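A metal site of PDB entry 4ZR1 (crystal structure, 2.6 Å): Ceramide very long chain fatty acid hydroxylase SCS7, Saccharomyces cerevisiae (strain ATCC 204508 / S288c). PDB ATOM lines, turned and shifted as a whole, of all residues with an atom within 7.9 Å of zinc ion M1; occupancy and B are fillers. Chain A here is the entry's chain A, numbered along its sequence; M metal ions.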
ATOM      1  N   HIS A  79     -33.618 -15.356   3.634  1.00  0.00           N
ATOM      2  CA  HIS A  79     -32.248 -15.037   4.043  1.00  0.00           C
ATOM      3  C   HIS A  79     -31.484 -14.287   2.940  1.00  0.00           C
ATOM      4  O   HIS A  79     -30.306 -13.974   3.098  1.00  0.00           O
ATOM      5  CB  HIS A  79     -31.480 -16.296   4.448  1.00  0.00           C
ATOM      6  CG  HIS A  79     -32.075 -17.020   5.614  1.00  0.00           C
ATOM      7  ND1 HIS A  79     -32.827 -18.172   5.479  1.00  0.00           N
ATOM      8  CD2 HIS A  79     -32.033 -16.755   6.944  1.00  0.00           C
ATOM      9  CE1 HIS A  79     -33.220 -18.577   6.668  1.00  0.00           C
ATOM     10  NE2 HIS A  79     -32.750 -17.738   7.574  1.00  0.00           N
ATOM     11  N   HIS A 150     -29.694 -18.796  18.556  1.00  0.00           N
ATOM     12  CA  HIS A 150     -29.388 -18.309  17.220  1.00  0.00           C
ATOM     13  C   HIS A 150     -29.211 -19.446  16.231  1.00  0.00           C
ATOM     14  O   HIS A 150     -29.793 -19.426  15.146  1.00  0.00           O
ATOM     15  CB  HIS A 150     -28.149 -17.445  17.236  1.00  0.00           C
ATOM     16  CG  HIS A 150     -27.929 -16.696  15.965  1.00  0.00           C
ATOM     17  ND1 HIS A 150     -26.792 -15.957  15.706  1.00  0.00           N
ATOM     18  CD2 HIS A 150     -28.719 -16.576  14.866  1.00  0.00           C
ATOM     19  CE1 HIS A 150     -26.884 -15.421  14.499  1.00  0.00           C
ATOM     20  NE2 HIS A 150     -28.040 -15.774  13.969  1.00  0.00           N
ATOM     21  N   ARG A 151     -28.410 -20.434  16.599  1.00  0.00           N
ATOM     22  CA  ARG A 151     -28.082 -21.527  15.670  1.00  0.00           C
ATOM     23  C   ARG A 151     -29.207 -22.546  15.502  1.00  0.00           C
ATOM     24  O   ARG A 151     -29.468 -23.009  14.383  1.00  0.00           O
ATOM     25  CB  ARG A 151     -26.820 -22.237  16.129  1.00  0.00           C
ATOM     26  CG  ARG A 151     -26.472 -23.456  15.302  1.00  0.00           C
ATOM     27  CD  ARG A 151     -25.146 -24.012  15.707  1.00  0.00           C
ATOM     28  NE  ARG A 151     -24.928 -25.356  15.173  1.00  0.00           N
ATOM     29  CZ  ARG A 151     -23.857 -26.091  15.449  1.00  0.00           C
ATOM     30  NH1 ARG A 151     -22.916 -25.613  16.264  1.00  0.00           N
ATOM     31  NH2 ARG A 151     -23.731 -27.293  14.920  1.00  0.00           N
ATOM     32  N   PHE A 154     -33.489 -19.946  15.995  1.00  0.00           N
ATOM     33  CA  PHE A 154     -33.570 -18.919  14.964  1.00  0.00           C
ATOM     34  C   PHE A 154     -33.256 -19.447  13.550  1.00  0.00           C
ATOM     35  O   PHE A 154     -33.913 -19.069  12.584  1.00  0.00           O
ATOM     36  CB  PHE A 154     -32.615 -17.779  15.298  1.00  0.00           C
ATOM     37  CG  PHE A 154     -33.056 -16.949  16.456  1.00  0.00           C
ATOM     38  CD1 PHE A 154     -34.239 -17.245  17.124  1.00  0.00           C
ATOM     39  CD2 PHE A 154     -32.292 -15.868  16.895  1.00  0.00           C
ATOM     40  CE1 PHE A 154     -34.653 -16.479  18.200  1.00  0.00           C
ATOM     41  CE2 PHE A 154     -32.719 -15.098  17.973  1.00  0.00           C
ATOM     42  CZ  PHE A 154     -33.884 -15.398  18.618  1.00  0.00           C
ATOM     43  N   HIS A 155     -32.257 -20.303  13.421  1.00  0.00           N
ATOM     44  CA  HIS A 155     -31.945 -20.853  12.111  1.00  0.00           C
ATOM     45  C   HIS A 155     -32.328 -22.328  11.989  1.00  0.00           C
ATOM     46  O   HIS A 155     -31.578 -23.118  11.437  1.00  0.00           O
ATOM     47  CB  HIS A 155     -30.456 -20.668  11.791  1.00  0.00           C
ATOM     48  CG  HIS A 155     -30.105 -19.247  11.449  1.00  0.00           C
ATOM     49  ND1 HIS A 155     -30.199 -18.756  10.172  1.00  0.00           N
ATOM     50  CD2 HIS A 155     -29.663 -18.233  12.225  1.00  0.00           C
ATOM     51  CE1 HIS A 155     -29.830 -17.486  10.166  1.00  0.00           C
ATOM     52  NE2 HIS A 155     -29.498 -17.138  11.400  1.00  0.00           N
ATOM     53  N   ASP A 157     -34.454 -23.347   9.926  1.00  0.00           N
ATOM     54  CA  ASP A 157     -34.306 -23.421   8.466  1.00  0.00           C
ATOM     55  C   ASP A 157     -34.723 -24.750   7.830  1.00  0.00           C
ATOM     56  O   ASP A 157     -35.910 -25.076   7.821  1.00  0.00           O
ATOM     57  CB  ASP A 157     -32.855 -23.107   8.081  1.00  0.00           C
ATOM     58  CG  ASP A 157     -32.414 -21.727   8.572  1.00  0.00           C
ATOM     59  OD1 ASP A 157     -33.243 -20.960   9.105  1.00  0.00           O
ATOM     60  OD2 ASP A 157     -31.220 -21.406   8.407  1.00  0.00           O
ATOM     61  N   HIS A 174     -36.621 -14.350  13.704  1.00  0.00           N
ATOM     62  CA  HIS A 174     -35.309 -14.051  13.148  1.00  0.00           C
ATOM     63  C   HIS A 174     -35.301 -13.860  11.621  1.00  0.00           C
ATOM     64  O   HIS A 174     -34.495 -13.104  11.088  1.00  0.00           O
ATOM     65  CB  HIS A 174     -34.331 -15.139  13.532  1.00  0.00           C
ATOM     66  CG  HIS A 174     -32.899 -14.748  13.374  1.00  0.00           C
ATOM     67  ND1 HIS A 174     -32.333 -13.695  14.061  1.00  0.00           N
ATOM     68  CD2 HIS A 174     -31.915 -15.256  12.594  1.00  0.00           C
ATOM     69  CE1 HIS A 174     -31.067 -13.575  13.720  1.00  0.00           C
ATOM     70  NE2 HIS A 174     -30.785 -14.515  12.829  1.00  0.00           N
ATOM     71  N   GLY A 175     -36.203 -14.559  10.916  1.00  0.00           N
ATOM     72  CA  GLY A 175     -36.246 -14.476   9.470  1.00  0.00           C
ATOM     73  C   GLY A 175     -36.369 -13.049   8.949  1.00  0.00           C
ATOM     74  O   GLY A 175     -35.663 -12.662   8.021  1.00  0.00           O
ATOM     75  N   HIS A 177     -35.402 -10.348  10.253  1.00  0.00           N
ATOM     76  CA  HIS A 177     -34.177  -9.606  10.446  1.00  0.00           C
ATOM     77  C   HIS A 177     -33.175  -9.920   9.312  1.00  0.00           C
ATOM     78  O   HIS A 177     -32.450  -9.034   8.846  1.00  0.00           O
ATOM     79  CB  HIS A 177     -33.586  -9.908  11.821  1.00  0.00           C
ATOM     80  CG  HIS A 177     -32.254  -9.274  12.041  1.00  0.00           C
ATOM     81  ND1 HIS A 177     -32.063  -7.909  11.968  1.00  0.00           N
ATOM     82  CD2 HIS A 177     -31.041  -9.812  12.277  1.00  0.00           C
ATOM     83  CE1 HIS A 177     -30.781  -7.641  12.176  1.00  0.00           C
ATOM     84  NE2 HIS A 177     -30.146  -8.772  12.365  1.00  0.00           N
ATOM     85  N   HIS A 178     -33.153 -11.167   8.863  1.00  0.00           N
ATOM     86  CA  HIS A 178     -32.323 -11.533   7.720  1.00  0.00           C
ATOM     87  C   HIS A 178     -32.916 -10.993   6.429  1.00  0.00           C
ATOM     88  O   HIS A 178     -32.188 -10.594   5.515  1.00  0.00           O
ATOM     89  CB  HIS A 178     -32.173 -13.051   7.624  1.00  0.00           C
ATOM     90  CG  HIS A 178     -31.007 -13.589   8.401  1.00  0.00           C
ATOM     91  ND1 HIS A 178     -29.845 -14.002   7.807  1.00  0.00           N
ATOM     92  CD2 HIS A 178     -30.835 -13.760   9.732  1.00  0.00           C
ATOM     93  CE1 HIS A 178     -28.993 -14.417   8.738  1.00  0.00           C
ATOM     94  NE2 HIS A 178     -29.576 -14.276   9.911  1.00  0.00           N
ATOM     95  N   TYR A 228     -26.187  -8.288  24.578  1.00  0.00           N
ATOM     96  CA  TYR A 228     -26.315  -8.919  23.260  1.00  0.00           C
ATOM     97  C   TYR A 228     -27.113  -8.094  22.232  1.00  0.00           C
ATOM     98  O   TYR A 228     -26.635  -7.837  21.123  1.00  0.00           O
ATOM     99  CB  TYR A 228     -26.965 -10.301  23.400  1.00  0.00           C
ATOM    100  CG  TYR A 228     -27.692 -10.746  22.145  1.00  0.00           C
ATOM    101  CD1 TYR A 228     -26.998 -11.283  21.067  1.00  0.00           C
ATOM    102  CD2 TYR A 228     -29.076 -10.641  22.032  1.00  0.00           C
ATOM    103  CE1 TYR A 228     -27.653 -11.690  19.912  1.00  0.00           C
ATOM    104  CE2 TYR A 228     -29.742 -11.048  20.907  1.00  0.00           C
ATOM    105  CZ  TYR A 228     -29.018 -11.565  19.836  1.00  0.00           C
ATOM    106  OH  TYR A 228     -29.685 -11.970  18.697  1.00  0.00           O
ATOM    107  N   HIS A 232     -25.841  -6.315  19.173  1.00  0.00           N
ATOM    108  CA  HIS A 232     -26.418  -6.717  17.899  1.00  0.00           C
ATOM    109  C   HIS A 232     -26.886  -5.515  17.086  1.00  0.00           C
ATOM    110  O   HIS A 232     -26.575  -5.403  15.912  1.00  0.00           O
ATOM    111  CB  HIS A 232     -27.578  -7.668  18.102  1.00  0.00           C
ATOM    112  CG  HIS A 232     -28.119  -8.223  16.832  1.00  0.00           C
ATOM    113  ND1 HIS A 232     -29.364  -8.809  16.748  1.00  0.00           N
ATOM    114  CD2 HIS A 232     -27.584  -8.286  15.595  1.00  0.00           C
ATOM    115  CE1 HIS A 232     -29.565  -9.205  15.497  1.00  0.00           C
ATOM    116  NE2 HIS A 232     -28.509  -8.887  14.777  1.00  0.00           N
ATOM    117  N   HIS A 251     -20.106 -10.505  12.107  1.00  0.00           N
ATOM    118  CA  HIS A 251     -21.545 -10.687  12.145  1.00  0.00           C
ATOM    119  C   HIS A 251     -22.206 -10.343  10.824  1.00  0.00           C
ATOM    120  O   HIS A 251     -23.131 -11.029  10.380  1.00  0.00           O
ATOM    121  CB  HIS A 251     -22.160  -9.839  13.254  1.00  0.00           C
ATOM    122  CG  HIS A 251     -23.647  -9.893  13.269  1.00  0.00           C
ATOM    123  ND1 HIS A 251     -24.342 -11.042  13.589  1.00  0.00           N
ATOM    124  CD2 HIS A 251     -24.578  -8.969  12.952  1.00  0.00           C
ATOM    125  CE1 HIS A 251     -25.634 -10.813  13.487  1.00  0.00           C
ATOM    126  NE2 HIS A 251     -25.812  -9.565  13.109  1.00  0.00           N
ATOM    127  N   HIS A 254     -22.258 -13.061   8.520  1.00  0.00           N
ATOM    128  CA  HIS A 254     -23.315 -14.007   8.816  1.00  0.00           C
ATOM    129  C   HIS A 254     -24.571 -13.648   8.013  1.00  0.00           C
ATOM    130  O   HIS A 254     -25.375 -14.507   7.644  1.00  0.00           O
ATOM    131  CB  HIS A 254     -23.628 -14.025  10.304  1.00  0.00           C
ATOM    132  CG  HIS A 254     -24.909 -14.709  10.646  1.00  0.00           C
ATOM    133  ND1 HIS A 254     -24.998 -16.082  10.824  1.00  0.00           N
ATOM    134  CD2 HIS A 254     -26.163 -14.234  10.811  1.00  0.00           C
ATOM    135  CE1 HIS A 254     -26.249 -16.403  11.086  1.00  0.00           C
ATOM    136  NE2 HIS A 254     -26.977 -15.301  11.086  1.00  0.00           N
ATOM    137  N   HIS A 255     -24.730 -12.365   7.747  1.00  0.00           N
ATOM    138  CA  HIS A 255     -25.842 -11.849   6.978  1.00  0.00           C
ATOM    139  C   HIS A 255     -25.595 -11.922   5.467  1.00  0.00           C
ATOM    140  O   HIS A 255     -26.414 -12.464   4.721  1.00  0.00           O
ATOM    141  CB  HIS A 255     -26.113 -10.396   7.388  1.00  0.00           C
ATOM    142  CG  HIS A 255     -26.882 -10.262   8.673  1.00  0.00           C
ATOM    143  ND1 HIS A 255     -28.232 -10.504   8.752  1.00  0.00           N
ATOM    144  CD2 HIS A 255     -26.478  -9.909   9.910  1.00  0.00           C
ATOM    145  CE1 HIS A 255     -28.638 -10.320  10.003  1.00  0.00           C
ATOM    146  NE2 HIS A 255     -27.595  -9.946  10.724  1.00  0.00           N
ATOM    147  N   ASN A 258     -22.601 -15.976   4.642  1.00  0.00           N
ATOM    148  CA  ASN A 258     -22.913 -17.329   5.105  1.00  0.00           C
ATOM    149  C   ASN A 258     -23.683 -17.316   6.424  1.00  0.00           C
ATOM    150  O   ASN A 258     -23.151 -16.892   7.454  1.00  0.00           O
ATOM    151  CB  ASN A 258     -21.622 -18.145   5.261  1.00  0.00           C
ATOM    152  CG  ASN A 258     -21.871 -19.648   5.326  1.00  0.00           C
ATOM    153  OD1 ASN A 258     -22.806 -20.110   5.974  1.00  0.00           O
ATOM    154  ND2 ASN A 258     -21.016 -20.420   4.647  1.00  0.00           N
ATOM    155  N   TYR A 259     -24.940 -17.764   6.396  1.00  0.00           N
ATOM    156  CA  TYR A 259     -25.752 -17.853   7.610  1.00  0.00           C
ATOM    157  C   TYR A 259     -25.836 -19.288   8.138  1.00  0.00           C
ATOM    158  O   TYR A 259     -26.719 -19.615   8.930  1.00  0.00           O
ATOM    159  CB  TYR A 259     -27.166 -17.282   7.364  1.00  0.00           C
ATOM    160  CG  TYR A 259     -28.007 -18.008   6.315  1.00  0.00           C
ATOM    161  CD1 TYR A 259     -27.877 -17.711   4.965  1.00  0.00           C
ATOM    162  CD2 TYR A 259     -28.962 -18.937   6.698  1.00  0.00           C
ATOM    163  CE1 TYR A 259     -28.649 -18.367   4.021  1.00  0.00           C
ATOM    164  CE2 TYR A 259     -29.747 -19.588   5.755  1.00  0.00           C
ATOM    165  CZ  TYR A 259     -29.587 -19.294   4.417  1.00  0.00           C
ATOM    166  OH  TYR A 259     -30.355 -19.942   3.488  1.00  0.00           O
ATOM    167  N   GLN A 260     -24.916 -20.142   7.678  1.00  0.00           N
ATOM    168  CA  GLN A 260     -24.753 -21.464   8.275  1.00  0.00           C
ATOM    169  C   GLN A 260     -23.607 -21.407   9.287  1.00  0.00           C
ATOM    170  O   GLN A 260     -23.307 -22.403   9.970  1.00  0.00           O
ATOM    171  CB  GLN A 260     -24.477 -22.532   7.210  1.00  0.00           C
ATOM    172  CG  GLN A 260     -25.706 -22.997   6.476  1.00  0.00           C
ATOM    173  CD  GLN A 260     -26.184 -22.011   5.426  1.00  0.00           C
ATOM    174  OE1 GLN A 260     -25.398 -21.527   4.605  1.00  0.00           O
ATOM    175  NE2 GLN A 260     -27.469 -21.702   5.456  1.00  0.00           N
ATOM    176  N   LEU A 261     -22.987 -20.235   9.392  1.00  0.00           N
ATOM    177  CA  LEU A 261     -21.885 -20.002  10.325  1.00  0.00           C
ATOM    178  C   LEU A 261     -22.042 -18.646  11.021  1.00  0.00           C
ATOM    179  O   LEU A 261     -22.952 -17.870  10.695  1.00  0.00           O
ATOM    180  CB  LEU A 261     -20.547 -20.047   9.583  1.00  0.00           C
ATOM    181  CG  LEU A 261     -20.233 -21.313   8.802  1.00  0.00           C
ATOM    182  CD1 LEU A 261     -19.011 -21.074   7.944  1.00  0.00           C
ATOM    183  CD2 LEU A 261     -20.006 -22.493   9.744  1.00  0.00           C
ATOM    184  N   GLY A 262     -21.153 -18.358  11.969  1.00  0.00           N
ATOM    185  CA  GLY A 262     -21.102 -17.064  12.620  1.00  0.00           C
ATOM    186  C   GLY A 262     -22.285 -16.776  13.542  1.00  0.00           C
ATOM    187  O   GLY A 262     -22.826 -15.659  13.545  1.00  0.00           O
ATOM    188  N   PHE A 263     -22.676 -17.770  14.326  1.00  0.00           N
ATOM    189  CA  PHE A 263     -23.850 -17.652  15.195  1.00  0.00           C
ATOM    190  C   PHE A 263     -23.586 -16.806  16.440  1.00  0.00           C
ATOM    191  O   PHE A 263     -24.530 -16.270  17.028  1.00  0.00           O
ATOM    192  CB  PHE A 263     -24.362 -19.028  15.583  1.00  0.00           C
ATOM    193  CG  PHE A 263     -24.729 -19.885  14.402  1.00  0.00           C
ATOM    194  CD1 PHE A 263     -25.818 -19.547  13.606  1.00  0.00           C
ATOM    195  CD2 PHE A 263     -23.984 -21.000  14.083  1.00  0.00           C
ATOM    196  CE1 PHE A 263     -26.167 -20.323  12.513  1.00  0.00           C
ATOM    197  CE2 PHE A 263     -24.327 -21.779  12.982  1.00  0.00           C
ATOM    198  CZ  PHE A 263     -25.415 -21.442  12.200  1.00  0.00           C
ATOM    199  N   VAL A 265     -22.645 -13.485  18.340  1.00  0.00           N
ATOM    200  CA  VAL A 265     -22.691 -12.089  17.924  1.00  0.00           C
ATOM    201  C   VAL A 265     -22.104 -11.174  18.997  1.00  0.00           C
ATOM    202  O   VAL A 265     -21.630 -10.070  18.681  1.00  0.00           O
ATOM    203  CB  VAL A 265     -24.168 -11.636  17.509  1.00  0.00           C
ATOM    204  CG1 VAL A 265     -25.107 -12.827  17.389  1.00  0.00           C
ATOM    205  CG2 VAL A 265     -24.745 -10.599  18.434  1.00  0.00           C
HETATM  206 ZN    ZN M   1     -28.960 -15.229  11.922  1.00  0.00          ZN
HETATM  207 ZN    ZN M   2     -27.925  -9.148  12.564  1.00  0.00          ZN
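OD2 of Asp 157 lies within hydrogen-bond range of ND1 of His 155, at 3.3 Å.
The backbone carbonyl oxygen (O) of Leu 261 is in hydrogen-bond range of a ring nitrogen (ND1) of His 254 (2.7 Å).
The backbone carbonyl oxygen (O) of Phe 263 is in hydrogen-bond range of a ring nitrogen (ND1) of His 150.
Of the 22 residues printed, 5 come within 4 Å of zinc ion M1.
The nearest printed residue that does not touch zinc ion M1 is His 255 (5.3 Å).
Zinc ion M1 is bound by NE2 of His 155, at 2.1 Å.
NE2 of His 254 is bound to zinc ion M1 (2.2 Å).
NE2 of His 174 is bound to zinc ion M1 (2.2 Å).
A ring nitrogen (NE2) of His 150 is bound to zinc ion M1 (2.3 Å).
NE2 of His 178 binds zinc ion M1, at 2.3 Å.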
